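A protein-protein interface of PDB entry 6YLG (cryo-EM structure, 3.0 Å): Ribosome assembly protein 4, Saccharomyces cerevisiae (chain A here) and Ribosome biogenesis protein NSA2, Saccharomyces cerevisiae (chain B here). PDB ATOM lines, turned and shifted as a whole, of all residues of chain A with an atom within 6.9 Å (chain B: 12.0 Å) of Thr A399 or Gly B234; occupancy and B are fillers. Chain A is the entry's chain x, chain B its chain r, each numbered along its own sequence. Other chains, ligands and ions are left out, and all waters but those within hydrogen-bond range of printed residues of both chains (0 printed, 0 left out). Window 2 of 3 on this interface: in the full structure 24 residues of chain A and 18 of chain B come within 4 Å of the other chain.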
ATOM      1  N   TYR A 381      -8.445 -10.967  -8.656  1.00  0.00           N
ATOM      2  CA  TYR A 381      -8.965 -10.852 -10.016  1.00  0.00           C
ATOM      3  C   TYR A 381      -9.680  -9.518 -10.204  1.00  0.00           C
ATOM      4  O   TYR A 381     -10.733  -9.438 -10.840  1.00  0.00           O
ATOM      5  CB  TYR A 381      -9.902 -12.017 -10.362  1.00  0.00           C
ATOM      6  CG  TYR A 381      -9.418 -13.409  -9.992  1.00  0.00           C
ATOM      7  CD1 TYR A 381      -8.069 -13.723  -9.955  1.00  0.00           C
ATOM      8  CD2 TYR A 381     -10.325 -14.414  -9.692  1.00  0.00           C
ATOM      9  CE1 TYR A 381      -7.638 -14.988  -9.624  1.00  0.00           C
ATOM     10  CE2 TYR A 381      -9.904 -15.681  -9.361  1.00  0.00           C
ATOM     11  CZ  TYR A 381      -8.558 -15.964  -9.329  1.00  0.00           C
ATOM     12  OH  TYR A 381      -8.128 -17.227  -8.999  1.00  0.00           O
ATOM     13  N   THR A 382      -9.099  -8.458  -9.646  1.00  0.00           N
ATOM     14  CA  THR A 382      -9.831  -7.206  -9.504  1.00  0.00           C
ATOM     15  C   THR A 382      -8.869  -6.036  -9.328  1.00  0.00           C
ATOM     16  O   THR A 382      -7.773  -6.185  -8.763  1.00  0.00           O
ATOM     17  CB  THR A 382     -10.793  -7.285  -8.308  1.00  0.00           C
ATOM     18  OG1 THR A 382     -11.714  -8.368  -8.490  1.00  0.00           O
ATOM     19  CG2 THR A 382     -11.587  -6.016  -8.152  1.00  0.00           C
ATOM     20  N   MET A 383      -9.305  -4.876  -9.824  1.00  0.00           N
ATOM     21  CA  MET A 383      -8.689  -3.584  -9.570  1.00  0.00           C
ATOM     22  C   MET A 383      -9.643  -2.702  -8.774  1.00  0.00           C
ATOM     23  O   MET A 383     -10.852  -2.935  -8.732  1.00  0.00           O
ATOM     24  CB  MET A 383      -8.336  -2.879 -10.882  1.00  0.00           C
ATOM     25  CG  MET A 383      -7.291  -3.562 -11.721  1.00  0.00           C
ATOM     26  SD  MET A 383      -7.438  -3.021 -13.423  1.00  0.00           S
ATOM     27  CE  MET A 383      -8.594  -4.233 -14.050  1.00  0.00           C
ATOM     28  N   ARG A 397     -14.812  -0.648  -8.423  1.00  0.00           N
ATOM     29  CA  ARG A 397     -14.134  -1.935  -8.328  1.00  0.00           C
ATOM     30  C   ARG A 397     -14.217  -2.586  -9.702  1.00  0.00           C
ATOM     31  O   ARG A 397     -15.259  -3.137 -10.067  1.00  0.00           O
ATOM     32  CB  ARG A 397     -14.784  -2.816  -7.260  1.00  0.00           C
ATOM     33  CG  ARG A 397     -14.120  -4.167  -7.072  1.00  0.00           C
ATOM     34  CD  ARG A 397     -14.711  -4.951  -5.907  1.00  0.00           C
ATOM     35  NE  ARG A 397     -13.773  -5.967  -5.432  1.00  0.00           N
ATOM     36  CZ  ARG A 397     -13.750  -6.485  -4.207  1.00  0.00           C
ATOM     37  NH1 ARG A 397     -14.620  -6.114  -3.276  1.00  0.00           N
ATOM     38  NH2 ARG A 397     -12.838  -7.399  -3.913  1.00  0.00           N
ATOM     39  N   MET A 398     -13.125  -2.523 -10.459  1.00  0.00           N
ATOM     40  CA  MET A 398     -13.117  -3.039 -11.824  1.00  0.00           C
ATOM     41  C   MET A 398     -12.919  -4.546 -11.782  1.00  0.00           C
ATOM     42  O   MET A 398     -11.857  -5.033 -11.369  1.00  0.00           O
ATOM     43  CB  MET A 398     -12.027  -2.379 -12.661  1.00  0.00           C
ATOM     44  CG  MET A 398     -11.872  -0.891 -12.447  1.00  0.00           C
ATOM     45  SD  MET A 398     -10.767  -0.152 -13.655  1.00  0.00           S
ATOM     46  CE  MET A 398      -9.578   0.590 -12.553  1.00  0.00           C
ATOM     47  N   THR A 399     -13.940  -5.273 -12.227  1.00  0.00           N
ATOM     48  CA  THR A 399     -13.962  -6.724 -12.279  1.00  0.00           C
ATOM     49  C   THR A 399     -14.120  -7.183 -13.720  1.00  0.00           C
ATOM     50  O   THR A 399     -14.547  -6.425 -14.594  1.00  0.00           O
ATOM     51  CB  THR A 399     -15.114  -7.292 -11.444  1.00  0.00           C
ATOM     52  OG1 THR A 399     -16.338  -7.188 -12.183  1.00  0.00           O
ATOM     53  CG2 THR A 399     -15.264  -6.533 -10.142  1.00  0.00           C
ATOM     54  N   GLY A 400     -13.793  -8.451 -13.947  1.00  0.00           N
ATOM     55  CA  GLY A 400     -13.959  -9.069 -15.247  1.00  0.00           C
ATOM     56  C   GLY A 400     -12.828 -10.008 -15.597  1.00  0.00           C
ATOM     57  O   GLY A 400     -13.018 -10.963 -16.357  1.00  0.00           O
ATOM     58  N   HIS A 401     -11.647  -9.758 -15.044  1.00  0.00           N
ATOM     59  CA  HIS A 401     -10.533 -10.673 -15.216  1.00  0.00           C
ATOM     60  C   HIS A 401     -10.836 -11.986 -14.512  1.00  0.00           C
ATOM     61  O   HIS A 401     -11.394 -12.002 -13.412  1.00  0.00           O
ATOM     62  CB  HIS A 401      -9.246 -10.063 -14.662  1.00  0.00           C
ATOM     63  CG  HIS A 401      -8.620  -9.052 -15.568  1.00  0.00           C
ATOM     64  ND1 HIS A 401      -8.222  -9.349 -16.852  1.00  0.00           N
ATOM     65  CD2 HIS A 401      -8.323  -7.747 -15.374  1.00  0.00           C
ATOM     66  CE1 HIS A 401      -7.704  -8.271 -17.410  1.00  0.00           C
ATOM     67  NE2 HIS A 401      -7.755  -7.284 -16.536  1.00  0.00           N
ATOM     68  N   LYS A 427      -7.214  -5.613 -20.680  1.00  0.00           N
ATOM     69  CA  LYS A 427      -8.528  -4.986 -20.619  1.00  0.00           C
ATOM     70  C   LYS A 427      -8.395  -3.480 -20.476  1.00  0.00           C
ATOM     71  O   LYS A 427      -7.529  -2.980 -19.748  1.00  0.00           O
ATOM     72  CB  LYS A 427      -9.349  -5.564 -19.470  1.00  0.00           C
ATOM     73  CG  LYS A 427      -9.857  -6.956 -19.779  1.00  0.00           C
ATOM     74  CD  LYS A 427     -10.854  -7.458 -18.763  1.00  0.00           C
ATOM     75  CE  LYS A 427     -11.351  -8.839 -19.140  1.00  0.00           C
ATOM     76  NZ  LYS A 427     -12.785  -8.836 -19.515  1.00  0.00           N
ATOM     77  N   TRP A 429     -10.047   0.375 -19.793  1.00  0.00           N
ATOM     78  CA  TRP A 429     -10.984   1.046 -18.908  1.00  0.00           C
ATOM     79  C   TRP A 429     -10.791   2.546 -19.067  1.00  0.00           C
ATOM     80  O   TRP A 429      -9.762   3.002 -19.566  1.00  0.00           O
ATOM     81  CB  TRP A 429     -10.773   0.635 -17.441  1.00  0.00           C
ATOM     82  CG  TRP A 429     -10.595  -0.842 -17.238  1.00  0.00           C
ATOM     83  CD1 TRP A 429      -9.456  -1.569 -17.430  1.00  0.00           C
ATOM     84  CD2 TRP A 429     -11.593  -1.772 -16.807  1.00  0.00           C
ATOM     85  NE1 TRP A 429      -9.684  -2.890 -17.152  1.00  0.00           N
ATOM     86  CE2 TRP A 429     -10.989  -3.042 -16.764  1.00  0.00           C
ATOM     87  CE3 TRP A 429     -12.938  -1.654 -16.453  1.00  0.00           C
ATOM     88  CZ2 TRP A 429     -11.681  -4.182 -16.382  1.00  0.00           C
ATOM     89  CZ3 TRP A 429     -13.623  -2.787 -16.077  1.00  0.00           C
ATOM     90  CH2 TRP A 429     -12.995  -4.034 -16.043  1.00  0.00           C
ATOM     91  N   GLY A 434     -13.913   4.274 -13.940  1.00  0.00           N
ATOM     92  CA  GLY A 434     -13.618   2.855 -13.888  1.00  0.00           C
ATOM     93  C   GLY A 434     -14.547   2.007 -14.719  1.00  0.00           C
ATOM     94  O   GLY A 434     -14.829   0.862 -14.349  1.00  0.00           O
ATOM     95  N   PHE A 436     -15.853  -0.104 -18.124  1.00  0.00           N
ATOM     96  CA  PHE A 436     -15.274  -1.012 -19.100  1.00  0.00           C
ATOM     97  C   PHE A 436     -15.332  -0.408 -20.496  1.00  0.00           C
ATOM     98  O   PHE A 436     -16.309   0.253 -20.859  1.00  0.00           O
ATOM     99  CB  PHE A 436     -16.020  -2.345 -19.077  1.00  0.00           C
ATOM    100  CG  PHE A 436     -15.409  -3.396 -19.944  1.00  0.00           C
ATOM    101  CD1 PHE A 436     -14.186  -3.952 -19.625  1.00  0.00           C
ATOM    102  CD2 PHE A 436     -16.057  -3.830 -21.082  1.00  0.00           C
ATOM    103  CE1 PHE A 436     -13.627  -4.919 -20.423  1.00  0.00           C
ATOM    104  CE2 PHE A 436     -15.500  -4.795 -21.882  1.00  0.00           C
ATOM    105  CZ  PHE A 436     -14.285  -5.341 -21.553  1.00  0.00           C
ATOM    106  N   GLY B 229     -14.209 -10.175   1.679  1.00  0.00           N
ATOM    107  CA  GLY B 229     -14.568  -9.329   0.560  1.00  0.00           C
ATOM    108  C   GLY B 229     -14.216  -9.938  -0.779  1.00  0.00           C
ATOM    109  O   GLY B 229     -13.879  -9.222  -1.726  1.00  0.00           O
ATOM    110  N   MET B 230     -14.296 -11.261  -0.872  1.00  0.00           N
ATOM    111  CA  MET B 230     -14.005 -11.944  -2.120  1.00  0.00           C
ATOM    112  C   MET B 230     -15.176 -11.794  -3.078  1.00  0.00           C
ATOM    113  O   MET B 230     -16.340 -11.786  -2.668  1.00  0.00           O
ATOM    114  CB  MET B 230     -13.717 -13.422  -1.868  1.00  0.00           C
ATOM    115  CG  MET B 230     -12.390 -13.664  -1.194  1.00  0.00           C
ATOM    116  SD  MET B 230     -12.451 -14.972   0.036  1.00  0.00           S
ATOM    117  CE  MET B 230     -11.996 -16.366  -0.983  1.00  0.00           C
ATOM    118  N   VAL B 231     -14.858 -11.670  -4.362  1.00  0.00           N
ATOM    119  CA  VAL B 231     -15.845 -11.416  -5.402  1.00  0.00           C
ATOM    120  C   VAL B 231     -15.387 -12.126  -6.666  1.00  0.00           C
ATOM    121  O   VAL B 231     -14.190 -12.131  -6.979  1.00  0.00           O
ATOM    122  CB  VAL B 231     -16.040  -9.910  -5.658  1.00  0.00           C
ATOM    123  CG1 VAL B 231     -14.721  -9.230  -6.009  1.00  0.00           C
ATOM    124  CG2 VAL B 231     -17.052  -9.682  -6.757  1.00  0.00           C
ATOM    125  N   THR B 232     -16.333 -12.717  -7.386  1.00  0.00           N
ATOM    126  CA  THR B 232     -16.015 -13.410  -8.624  1.00  0.00           C
ATOM    127  C   THR B 232     -16.078 -12.449  -9.804  1.00  0.00           C
ATOM    128  O   THR B 232     -16.564 -11.320  -9.691  1.00  0.00           O
ATOM    129  CB  THR B 232     -16.987 -14.572  -8.840  1.00  0.00           C
ATOM    130  OG1 THR B 232     -16.464 -15.462  -9.833  1.00  0.00           O
ATOM    131  CG2 THR B 232     -18.355 -14.068  -9.277  1.00  0.00           C
ATOM    132  N   ALA B 233     -15.580 -12.908 -10.947  1.00  0.00           N
ATOM    133  CA  ALA B 233     -15.752 -12.170 -12.189  1.00  0.00           C
ATOM    134  C   ALA B 233     -17.235 -12.095 -12.515  1.00  0.00           C
ATOM    135  O   ALA B 233     -17.891 -13.128 -12.687  1.00  0.00           O
ATOM    136  CB  ALA B 233     -14.983 -12.844 -13.318  1.00  0.00           C
ATOM    137  N   GLY B 234     -17.760 -10.872 -12.610  1.00  0.00           N
ATOM    138  CA  GLY B 234     -19.189 -10.615 -12.682  1.00  0.00           C
ATOM    139  C   GLY B 234     -19.700  -9.750 -11.547  1.00  0.00           C
ATOM    140  O   GLY B 234     -20.774  -9.152 -11.665  1.00  0.00           O
ATOM    141  N   GLY B 235     -18.952  -9.678 -10.448  1.00  0.00           N
ATOM    142  CA  GLY B 235     -19.319  -8.835  -9.330  1.00  0.00           C
ATOM    143  C   GLY B 235     -20.143  -9.510  -8.261  1.00  0.00           C
ATOM    144  O   GLY B 235     -20.636  -8.829  -7.356  1.00  0.00           O
ATOM    145  N   LYS B 236     -20.308 -10.827  -8.331  1.00  0.00           N
ATOM    146  CA  LYS B 236     -21.035 -11.573  -7.316  1.00  0.00           C
ATOM    147  C   LYS B 236     -20.126 -11.841  -6.128  1.00  0.00           C
ATOM    148  O   LYS B 236     -19.039 -12.406  -6.279  1.00  0.00           O
ATOM    149  CB  LYS B 236     -21.551 -12.900  -7.868  1.00  0.00           C
ATOM    150  CG  LYS B 236     -22.203 -12.803  -9.222  1.00  0.00           C
ATOM    151  CD  LYS B 236     -23.148 -13.967  -9.441  1.00  0.00           C
ATOM    152  CE  LYS B 236     -23.739 -13.947 -10.831  1.00  0.00           C
ATOM    153  NZ  LYS B 236     -24.930 -14.826 -10.921  1.00  0.00           N
ATOM    154  N   VAL B 237     -20.581 -11.456  -4.957  1.00  0.00           N
ATOM    155  CA  VAL B 237     -19.804 -11.634  -3.739  1.00  0.00           C
ATOM    156  C   VAL B 237     -19.849 -13.099  -3.341  1.00  0.00           C
ATOM    157  O   VAL B 237     -20.910 -13.734  -3.351  1.00  0.00           O
ATOM    158  CB  VAL B 237     -20.325 -10.722  -2.610  1.00  0.00           C
ATOM    159  CG1 VAL B 237     -21.698 -11.163  -2.139  1.00  0.00           C
ATOM    160  CG2 VAL B 237     -19.344 -10.705  -1.447  1.00  0.00           C
ATOM    161  N   VAL B 238     -18.685 -13.643  -3.007  1.00  0.00           N
ATOM    162  CA  VAL B 238     -18.557 -15.005  -2.514  1.00  0.00           C
ATOM    163  C   VAL B 238     -18.734 -14.971  -1.005  1.00  0.00           C
ATOM    164  O   VAL B 238     -18.150 -14.123  -0.324  1.00  0.00           O
ATOM    165  CB  VAL B 238     -17.198 -15.628  -2.890  1.00  0.00           C
ATOM    166  CG1 VAL B 238     -17.058 -16.997  -2.261  1.00  0.00           C
ATOM    167  CG2 VAL B 238     -17.051 -15.711  -4.394  1.00  0.00           C
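O of Gly B229 is in hydrogen-bond range of NH2 of Arg A397.
Among the printed residues, pairs that only touch across the chains: Thr A382 with Val B231 (3.99 Å), Arg A397 with Val B231 (3.4 Å), Thr A399 with Gly B234 (3.97 Å) and His A401 with Ala B233 (3.7 Å).
Printed residues of chain B within 4 Å of Thr A382: Val B231. Of chain B, only Gly B229 (3.0 Å) and Val B231 (3.4 Å) come within 4 Å of Arg A397. No residue of chain B comes within 4 Å of Met A398. Of the printed residues of chain B, Thr A399 touches Gly B234. Printed residues of chain A within 4 Å of Gly B229: Arg A397 (3.0 Å). Met B230 touches none of the printed residues of chain A. Printed residues of chain A within 4 Å of Val B231: Thr A382 (3.99 Å) and Arg A397 (3.4 Å). Printed residues of chain A within 4 Å of Ala B233: His A401. Of chain A, only Thr A399 (3.97 Å) comes within 4 Å of Gly B234. The nearest printed residue of chain B that does not touch Thr A399 is Gly B235 (4.01 Å). The nearest residue of chain A that does not touch Gly B234 is Gly A400 (4.8 Å).
Printed residues of chain A that touch a printed residue of chain B: Thr A382, Arg A397, Thr A399 and His A401. Printed residues of chain B that touch a printed residue of chain A: Gly B229, Val B231, Ala B233 and Gly B234. Hydrophobic or aromatic side chains of chain B that line the printed part of chain A: Val B231 and Ala B233. Along chain B the printed residues that touch a printed residue of chain A span positions 229 to 234.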
